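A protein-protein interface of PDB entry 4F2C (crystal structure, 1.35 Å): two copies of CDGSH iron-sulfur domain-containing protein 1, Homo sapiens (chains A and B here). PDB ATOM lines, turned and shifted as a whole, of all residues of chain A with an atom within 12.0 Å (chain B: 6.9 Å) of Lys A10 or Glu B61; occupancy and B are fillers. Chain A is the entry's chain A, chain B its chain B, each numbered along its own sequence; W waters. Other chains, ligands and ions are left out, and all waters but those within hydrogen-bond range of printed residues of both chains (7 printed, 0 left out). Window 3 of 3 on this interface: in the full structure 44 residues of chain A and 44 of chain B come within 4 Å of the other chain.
NZ of Lys A10 lies within salt-bridge range of OE2 of Glu B61 (2.8 Å). N of Ile A13 sits at hydrogen-bond distance from OD2 of Asp B64 (2.7 Å). OD2 of Asp B64 is in hydrogen-bond range of N of Asn A14 (3.1 Å). The side-chain amino group (NZ) of Lys A19 is in salt-bridge range of the side-chain carboxylate (OD1) of Asp B64, at 2.9 Å.
NZ of Lys A19 lies within hydrogen-bond range of SD of Met A12 (3.7 Å). The backbone carbonyl oxygen (O) of Ile A13 lies within hydrogen-bond range of the guanidinium group (NH1) of Arg A44, at 2.8 Å. NZ of Lys A19 sits at hydrogen-bond distance from O of Asn A14, 2.8 Å away. The side-chain amino group (NZ) of Lys B57 is in salt-bridge range of the side-chain carboxylate (OE1) of Glu B61, 3.6 Å away. The backbone carbonyl oxygen (O) of Asp B64 lies close to the side-chain amide oxygen (OD1) of Asn B59. N of Asp B64 lies close to OG1 of Thr B62 (3.2 Å).
Among the printed residues, pairs that only touch across the chains: Met A12 with Thr B62 (3.4 Å), Met A12 with Gly B63 (3.4 Å), Ile A13 with His B58 (3.5 Å), Ala A11 with Thr B62 (3.6 Å), Met A12 with Asp B64 (3.7 Å), Ala A11 with His B58 (3.7 Å), Lys A10 with Thr B62 (3.8 Å) and Ile A13 with Arg B44 (3.8 Å).
Printed residues of chain B within 4 Å of Lys A10: Glu B61 and Thr B62. Of the printed residues of chain B, Ala A11 touches His B58 (3.7 Å) and Thr B62 (3.6 Å). Of the printed residues of chain B, Asn A14 touches Asp B64. No residue of chain A comes within 4 Å of Lys B57. Of the printed residues of chain A, Glu B61 touches Lys A10 (2.8 Å). The nearest printed residue of chain B that does not touch Ala A11 is Arg B44 (5.0 Å).
Of the 12 printed residues of chain A, 6 touch a printed residue of chain B. Along chain B the printed residues that touch a printed residue of chain A span positions 44 to 64.
2 positions are printed for both chains. Of the 12 pairs that touch across the chains among the printed residues, none has its exchanged pair printed and touching as well.
Water W4 lies within hydrogen-bond range of O of Thr B62 (2.7 Å) and O of Lys A10 (3.4 Å). Water W2 lies within hydrogen-bond range of the backbone carbonyl oxygen of Gly B63 (2.7 Å), the side-chain amino group of Lys A19 (2.8 Å) and the side-chain sulfur of Met A12 (3.8 Å). Water W6 lies within hydrogen-bond range of OG1 of Thr B56 (2.7 Å) and NZ of Lys A23 (3.4 Å). Water W7 bridges the side-chain carboxylate of Glu B61 (2.8 Å) and the backbone NH of Lys A10 (2.9 Å). Water W3 bridges O of Ala A11 (2.9 Å) and NH2 of Arg B44 (2.9 Å). Water W5 bridges the guanidinium group of Arg B44 (3.4 Å) and the backbone carbonyl oxygen of Ala A11 (3.4 Å).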
ATOM      1  N   ARG A   8       6.937  30.729  -6.901  1.00  0.00           N
ATOM      2  CA  ARG A   8       7.099  29.310  -6.586  1.00  0.00           C
ATOM      3  C   ARG A   8       7.398  28.457  -7.813  1.00  0.00           C
ATOM      4  O   ARG A   8       8.141  27.474  -7.726  1.00  0.00           O
ATOM      5  CB  ARG A   8       5.860  28.773  -5.869  1.00  0.00           C
ATOM      6  CG  ARG A   8       5.843  29.063  -4.385  1.00  0.00           C
ATOM      7  CD  ARG A   8       4.478  28.759  -3.792  1.00  0.00           C
ATOM      8  NE  ARG A   8       3.506  29.807  -4.098  1.00  0.00           N
ATOM      9  CZ  ARG A   8       2.255  29.821  -3.644  1.00  0.00           C
ATOM     10  NH1 ARG A   8       1.810  28.837  -2.867  1.00  0.00           N
ATOM     11  NH2 ARG A   8       1.444  30.823  -3.968  1.00  0.00           N
ATOM     12  N   ASN A   9       6.808  28.828  -8.947  1.00  0.00           N
ATOM     13  CA  ASN A   9       7.067  28.148 -10.211  1.00  0.00           C
ATOM     14  C   ASN A   9       8.242  28.752 -10.954  1.00  0.00           C
ATOM     15  O   ASN A   9       8.345  29.974 -11.083  1.00  0.00           O
ATOM     16  CB  ASN A   9       5.829  28.179 -11.095  1.00  0.00           C
ATOM     17  CG  ASN A   9       4.669  27.459 -10.465  1.00  0.00           C
ATOM     18  OD1 ASN A   9       4.855  26.435  -9.794  1.00  0.00           O
ATOM     19  ND2 ASN A   9       3.461  27.980 -10.667  1.00  0.00           N
ATOM     20  N   LYS A  10       9.125  27.888 -11.443  1.00  0.00           N
ATOM     21  CA  LYS A  10      10.339  28.347 -12.108  1.00  0.00           C
ATOM     22  C   LYS A  10      10.030  29.125 -13.377  1.00  0.00           C
ATOM     23  O   LYS A  10       9.123  28.775 -14.137  1.00  0.00           O
ATOM     24  CB  LYS A  10      11.278  27.177 -12.394  1.00  0.00           C
ATOM     25  CG  LYS A  10      11.912  26.572 -11.139  1.00  0.00           C
ATOM     26  CD  LYS A  10      13.221  25.870 -11.482  1.00  0.00           C
ATOM     27  CE  LYS A  10      13.862  25.248 -10.251  1.00  0.00           C
ATOM     28  NZ  LYS A  10      13.026  24.159  -9.693  1.00  0.00           N
ATOM     29  N   ALA A  11      10.787  30.194 -13.589  1.00  0.00           N
ATOM     30  CA  ALA A  11      10.573  31.075 -14.727  1.00  0.00           C
ATOM     31  C   ALA A  11      11.319  30.604 -15.967  1.00  0.00           C
ATOM     32  O   ALA A  11      12.384  29.990 -15.869  1.00  0.00           O
ATOM     33  CB  ALA A  11      11.024  32.482 -14.382  1.00  0.00           C
ATOM     34  N   MET A  12      10.772  30.906 -17.140  1.00  0.00           N
ATOM     35  CA  MET A  12      11.530  30.744 -18.373  1.00  0.00           C
ATOM     36  C   MET A  12      12.722  31.691 -18.348  1.00  0.00           C
ATOM     37  O   MET A  12      12.702  32.720 -17.655  1.00  0.00           O
ATOM     38  CB  MET A  12      10.679  31.056 -19.605  1.00  0.00           C
ATOM     39  CG  MET A  12       9.558  30.075 -19.864  1.00  0.00           C
ATOM     40  SD  MET A  12       8.796  30.356 -21.481  1.00  0.00           S
ATOM     41  CE  MET A  12       7.373  29.276 -21.359  1.00  0.00           C
ATOM     42  N   ILE A  13      13.756  31.323 -19.084  1.00  0.00           N
ATOM     43  CA  ILE A  13      14.916  32.168 -19.297  1.00  0.00           C
ATOM     44  C   ILE A  13      14.694  33.035 -20.526  1.00  0.00           C
ATOM     45  O   ILE A  13      14.920  34.242 -20.489  1.00  0.00           O
ATOM     46  CB  ILE A  13      16.160  31.287 -19.465  1.00  0.00           C
ATOM     47  CG1 ILE A  13      16.568  30.746 -18.086  1.00  0.00           C
ATOM     48  CG2 ILE A  13      17.280  32.037 -20.166  1.00  0.00           C
ATOM     49  CD1 ILE A  13      17.528  29.597 -18.158  1.00  0.00           C
ATOM     50  N   ASN A  14      14.229  32.411 -21.612  1.00  0.00           N
ATOM     51  CA  ASN A  14      13.932  33.131 -22.835  1.00  0.00           C
ATOM     52  C   ASN A  14      12.457  33.534 -22.840  1.00  0.00           C
ATOM     53  O   ASN A  14      11.584  32.677 -22.847  1.00  0.00           O
ATOM     54  CB  ASN A  14      14.242  32.242 -24.043  1.00  0.00           C
ATOM     55  CG  ASN A  14      13.810  32.870 -25.343  1.00  0.00           C
ATOM     56  OD1 ASN A  14      13.796  34.102 -25.477  1.00  0.00           O
ATOM     57  ND2 ASN A  14      13.450  32.031 -26.314  1.00  0.00           N
ATOM     58  N   LEU A  15      12.175  34.832 -22.822  1.00  0.00           N
ATOM     59  CA  LEU A  15      10.786  35.275 -22.779  1.00  0.00           C
ATOM     60  C   LEU A  15      10.127  35.348 -24.156  1.00  0.00           C
ATOM     61  O   LEU A  15       8.928  35.056 -24.298  1.00  0.00           O
ATOM     62  CB  LEU A  15      10.700  36.647 -22.113  1.00  0.00           C
ATOM     63  CG  LEU A  15      11.248  36.689 -20.687  1.00  0.00           C
ATOM     64  CD1 LEU A  15      11.206  38.099 -20.147  1.00  0.00           C
ATOM     65  CD2 LEU A  15      10.441  35.752 -19.818  1.00  0.00           C
ATOM     66  N   LYS A  19       9.826  31.775 -30.474  1.00  0.00           N
ATOM     67  CA  LYS A  19       9.029  30.824 -29.714  1.00  0.00           C
ATOM     68  C   LYS A  19       8.408  29.707 -30.564  1.00  0.00           C
ATOM     69  O   LYS A  19       7.905  28.732 -30.021  1.00  0.00           O
ATOM     70  CB  LYS A  19       8.011  31.563 -28.833  1.00  0.00           C
ATOM     71  CG  LYS A  19       8.695  32.264 -27.631  1.00  0.00           C
ATOM     72  CD  LYS A  19       9.434  31.245 -26.775  1.00  0.00           C
ATOM     73  CE  LYS A  19       9.988  31.841 -25.462  1.00  0.00           C
ATOM     74  NZ  LYS A  19      10.642  30.783 -24.617  1.00  0.00           N
ATOM     75  N   PRO A  22      11.152  24.865 -31.126  1.00  0.00           N
ATOM     76  CA  PRO A  22      11.051  24.170 -29.827  1.00  0.00           C
ATOM     77  C   PRO A  22      12.353  24.092 -29.026  1.00  0.00           C
ATOM     78  O   PRO A  22      12.306  23.832 -27.829  1.00  0.00           O
ATOM     79  CB  PRO A  22      10.576  22.768 -30.210  1.00  0.00           C
ATOM     80  CG  PRO A  22      10.979  22.616 -31.649  1.00  0.00           C
ATOM     81  CD  PRO A  22      10.897  23.970 -32.269  1.00  0.00           C
ATOM     82  N   LYS A  23      13.488  24.306 -29.674  1.00  0.00           N
ATOM     83  CA  LYS A  23      14.760  24.319 -28.966  1.00  0.00           C
ATOM     84  C   LYS A  23      15.762  25.085 -29.798  1.00  0.00           C
ATOM     85  O   LYS A  23      16.162  24.643 -30.879  1.00  0.00           O
ATOM     86  CB  LYS A  23      15.285  22.911 -28.691  1.00  0.00           C
ATOM     87  CG  LYS A  23      16.584  22.940 -27.863  1.00  0.00           C
ATOM     88  CD  LYS A  23      17.072  21.553 -27.494  1.00  0.00           C
ATOM     89  CE  LYS A  23      17.411  20.745 -28.720  1.00  0.00           C
ATOM     90  NZ  LYS A  23      18.012  19.427 -28.356  1.00  0.00           N
ATOM     91  N   ARG A  44      18.082  38.290 -24.213  1.00  0.00           N
ATOM     92  CA  ARG A  44      17.415  39.585 -24.298  1.00  0.00           C
ATOM     93  C   ARG A  44      17.924  40.417 -25.472  1.00  0.00           C
ATOM     94  O   ARG A  44      17.381  41.474 -25.751  1.00  0.00           O
ATOM     95  CB  ARG A  44      17.573  40.381 -23.003  1.00  0.00           C
ATOM     96  CG  ARG A  44      17.053  39.678 -21.762  1.00  0.00           C
ATOM     97  CD  ARG A  44      15.525  39.592 -21.747  1.00  0.00           C
ATOM     98  NE  ARG A  44      15.096  38.913 -20.527  1.00  0.00           N
ATOM     99  CZ  ARG A  44      14.969  37.594 -20.419  1.00  0.00           C
ATOM    100  NH1 ARG A  44      15.169  36.803 -21.479  1.00  0.00           N
ATOM    101  NH2 ARG A  44      14.614  37.056 -19.262  1.00  0.00           N
ATOM    102  N   LEU B  15      20.643  31.474 -11.490  1.00  0.00           N
ATOM    103  CA  LEU B  15      20.206  31.348 -10.109  1.00  0.00           C
ATOM    104  C   LEU B  15      21.362  31.168  -9.129  1.00  0.00           C
ATOM    105  O   LEU B  15      21.303  31.679  -8.006  1.00  0.00           O
ATOM    106  CB  LEU B  15      19.224  30.173  -9.970  1.00  0.00           C
ATOM    107  CG  LEU B  15      17.983  30.279 -10.856  1.00  0.00           C
ATOM    108  CD1 LEU B  15      17.090  29.049 -10.713  1.00  0.00           C
ATOM    109  CD2 LEU B  15      17.223  31.547 -10.511  1.00  0.00           C
ATOM    110  N   HIS B  16      22.412  30.456  -9.541  1.00  0.00           N
ATOM    111  CA  HIS B  16      23.411  29.968  -8.585  1.00  0.00           C
ATOM    112  C   HIS B  16      24.872  30.079  -9.000  1.00  0.00           C
ATOM    113  O   HIS B  16      25.752  29.837  -8.178  1.00  0.00           O
ATOM    114  CB  HIS B  16      23.140  28.493  -8.265  1.00  0.00           C
ATOM    115  CG  HIS B  16      21.760  28.228  -7.753  1.00  0.00           C
ATOM    116  ND1 HIS B  16      20.911  27.314  -8.340  1.00  0.00           N
ATOM    117  CD2 HIS B  16      21.082  28.750  -6.702  1.00  0.00           C
ATOM    118  CE1 HIS B  16      19.770  27.285  -7.675  1.00  0.00           C
ATOM    119  NE2 HIS B  16      19.845  28.150  -6.680  1.00  0.00           N
ATOM    120  N   ARG B  44      22.253  26.503 -16.261  1.00  0.00           N
ATOM    121  CA  ARG B  44      21.873  25.387 -15.387  1.00  0.00           C
ATOM    122  C   ARG B  44      22.878  24.244 -15.422  1.00  0.00           C
ATOM    123  O   ARG B  44      22.774  23.302 -14.632  1.00  0.00           O
ATOM    124  CB  ARG B  44      20.484  24.843 -15.764  1.00  0.00           C
ATOM    125  CG  ARG B  44      19.369  25.870 -15.702  1.00  0.00           C
ATOM    126  CD  ARG B  44      19.013  26.252 -14.278  1.00  0.00           C
ATOM    127  NE  ARG B  44      17.933  27.236 -14.279  1.00  0.00           N
ATOM    128  CZ  ARG B  44      18.136  28.548 -14.367  1.00  0.00           C
ATOM    129  NH1 ARG B  44      19.377  29.016 -14.425  1.00  0.00           N
ATOM    130  NH2 ARG B  44      17.119  29.392 -14.378  1.00  0.00           N
ATOM    131  N   HIS B  55      19.804  21.903 -20.039  1.00  0.00           N
ATOM    132  CA  HIS B  55      18.765  22.688 -20.696  1.00  0.00           C
ATOM    133  C   HIS B  55      17.492  21.878 -20.955  1.00  0.00           C
ATOM    134  O   HIS B  55      16.396  22.438 -20.987  1.00  0.00           O
ATOM    135  CB  HIS B  55      19.282  23.292 -22.004  1.00  0.00           C
ATOM    136  CG  HIS B  55      19.780  22.274 -22.975  1.00  0.00           C
ATOM    137  ND1 HIS B  55      21.118  21.964 -23.108  1.00  0.00           N
ATOM    138  CD2 HIS B  55      19.117  21.476 -23.844  1.00  0.00           C
ATOM    139  CE1 HIS B  55      21.253  21.023 -24.029  1.00  0.00           C
ATOM    140  NE2 HIS B  55      20.054  20.709 -24.486  1.00  0.00           N
ATOM    141  N   THR B  56      17.637  20.567 -21.142  1.00  0.00           N
ATOM    142  CA  THR B  56      16.476  19.726 -21.421  1.00  0.00           C
ATOM    143  C   THR B  56      15.498  19.739 -20.248  1.00  0.00           C
ATOM    144  O   THR B  56      14.297  19.966 -20.426  1.00  0.00           O
ATOM    145  CB  THR B  56      16.899  18.286 -21.748  1.00  0.00           C
ATOM    146  OG1 THR B  56      17.820  18.308 -22.847  1.00  0.00           O
ATOM    147  CG2 THR B  56      15.678  17.438 -22.111  1.00  0.00           C
ATOM    148  N   LYS B  57      16.012  19.527 -19.039  1.00  0.00           N
ATOM    149  CA  LYS B  57      15.166  19.581 -17.849  1.00  0.00           C
ATOM    150  C   LYS B  57      14.595  20.977 -17.640  1.00  0.00           C
ATOM    151  O   LYS B  57      13.435  21.129 -17.276  1.00  0.00           O
ATOM    152  CB  LYS B  57      15.937  19.130 -16.609  1.00  0.00           C
ATOM    153  CG  LYS B  57      15.141  19.240 -15.322  1.00  0.00           C
ATOM    154  CD  LYS B  57      15.928  18.665 -14.160  1.00  0.00           C
ATOM    155  CE  LYS B  57      15.142  18.732 -12.866  1.00  0.00           C
ATOM    156  NZ  LYS B  57      15.020  20.127 -12.362  1.00  0.00           N
ATOM    157  N   HIS B  58      15.409  22.003 -17.879  1.00  0.00           N
ATOM    158  CA  HIS B  58      14.916  23.361 -17.745  1.00  0.00           C
ATOM    159  C   HIS B  58      13.732  23.610 -18.678  1.00  0.00           C
ATOM    160  O   HIS B  58      12.724  24.187 -18.269  1.00  0.00           O
ATOM    161  CB  HIS B  58      16.011  24.373 -18.048  1.00  0.00           C
ATOM    162  CG  HIS B  58      15.478  25.748 -18.275  1.00  0.00           C
ATOM    163  ND1 HIS B  58      15.063  26.571 -17.248  1.00  0.00           N
ATOM    164  CD2 HIS B  58      15.236  26.424 -19.423  1.00  0.00           C
ATOM    165  CE1 HIS B  58      14.612  27.706 -17.756  1.00  0.00           C
ATOM    166  NE2 HIS B  58      14.704  27.641 -19.074  1.00  0.00           N
ATOM    167  N   ASN B  59      13.868  23.206 -19.937  1.00  0.00           N
ATOM    168  CA  ASN B  59      12.804  23.413 -20.906  1.00  0.00           C
ATOM    169  C   ASN B  59      11.560  22.625 -20.517  1.00  0.00           C
ATOM    170  O   ASN B  59      10.441  23.118 -20.644  1.00  0.00           O
ATOM    171  CB  ASN B  59      13.264  23.029 -22.313  1.00  0.00           C
ATOM    172  CG  ASN B  59      14.271  24.020 -22.894  1.00  0.00           C
ATOM    173  OD1 ASN B  59      14.357  25.173 -22.450  1.00  0.00           O
ATOM    174  ND2 ASN B  59      15.038  23.576 -23.895  1.00  0.00           N
ATOM    175  N   GLU B  60      11.757  21.408 -20.019  1.00  0.00           N
ATOM    176  CA  GLU B  60      10.640  20.569 -19.597  1.00  0.00           C
ATOM    177  C   GLU B  60       9.881  21.192 -18.424  1.00  0.00           C
ATOM    178  O   GLU B  60       8.656  21.268 -18.435  1.00  0.00           O
ATOM    179  CB  GLU B  60      11.149  19.177 -19.214  1.00  0.00           C
ATOM    180  CG  GLU B  60      10.060  18.157 -18.958  1.00  0.00           C
ATOM    181  CD  GLU B  60      10.618  16.771 -18.696  1.00  0.00           C
ATOM    182  OE1 GLU B  60      11.276  16.213 -19.600  1.00  0.00           O
ATOM    183  OE2 GLU B  60      10.400  16.236 -17.586  1.00  0.00           O
ATOM    184  N   GLU B  61      10.625  21.651 -17.418  1.00  0.00           N
ATOM    185  CA  GLU B  61       9.998  22.199 -16.223  1.00  0.00           C
ATOM    186  C   GLU B  61       9.319  23.549 -16.449  1.00  0.00           C
ATOM    187  O   GLU B  61       8.281  23.822 -15.849  1.00  0.00           O
ATOM    188  CB  GLU B  61      11.005  22.309 -15.076  1.00  0.00           C
ATOM    189  CG  GLU B  61      10.435  22.994 -13.839  1.00  0.00           C
ATOM    190  CD  GLU B  61      11.435  23.113 -12.709  1.00  0.00           C
ATOM    191  OE1 GLU B  61      12.619  22.763 -12.911  1.00  0.00           O
ATOM    192  OE2 GLU B  61      11.031  23.559 -11.615  1.00  0.00           O
ATOM    193  N   THR B  62       9.889  24.380 -17.316  1.00  0.00           N
ATOM    194  CA  THR B  62       9.419  25.756 -17.478  1.00  0.00           C
ATOM    195  C   THR B  62       8.656  26.036 -18.769  1.00  0.00           C
ATOM    196  O   THR B  62       8.046  27.091 -18.898  1.00  0.00           O
ATOM    197  CB  THR B  62      10.595  26.752 -17.426  1.00  0.00           C
ATOM    198  OG1 THR B  62      11.432  26.555 -18.576  1.00  0.00           O
ATOM    199  CG2 THR B  62      11.405  26.560 -16.145  1.00  0.00           C
ATOM    200  N   GLY B  63       8.713  25.109 -19.721  1.00  0.00           N
ATOM    201  CA  GLY B  63       8.100  25.314 -21.019  1.00  0.00           C
ATOM    202  C   GLY B  63       8.959  26.146 -21.957  1.00  0.00           C
ATOM    203  O   GLY B  63       8.501  26.570 -23.011  1.00  0.00           O
ATOM    204  N   ASP B  64      10.210  26.381 -21.571  1.00  0.00           N
ATOM    205  CA  ASP B  64      11.135  27.201 -22.352  1.00  0.00           C
ATOM    206  C   ASP B  64      11.659  26.441 -23.569  1.00  0.00           C
ATOM    207  O   ASP B  64      11.366  25.250 -23.773  1.00  0.00           O
ATOM    208  CB  ASP B  64      12.316  27.613 -21.448  1.00  0.00           C
ATOM    209  CG  ASP B  64      12.940  28.953 -21.838  1.00  0.00           C
ATOM    210  OD1 ASP B  64      12.615  29.525 -22.906  1.00  0.00           O
ATOM    211  OD2 ASP B  64      13.782  29.435 -21.042  1.00  0.00           O
HETATM  212  O   HOH W   1       7.092  26.561 -14.331  1.00  0.00           O
HETATM  213  O   HOH W   2       8.868  28.561 -24.804  1.00  0.00           O
HETATM  214  O   HOH W   3      14.278  28.849 -14.010  1.00  0.00           O
HETATM  215  O   HOH W   4       7.363  28.911 -17.090  1.00  0.00           O
HETATM  216  O   HOH W   5      14.990  31.967 -14.867  1.00  0.00           O
HETATM  217  O   HOH W   6      16.701  18.985 -25.234  1.00  0.00           O
HETATM  218  O   HOH W   7       8.696  25.031 -11.264  1.00  0.00           O
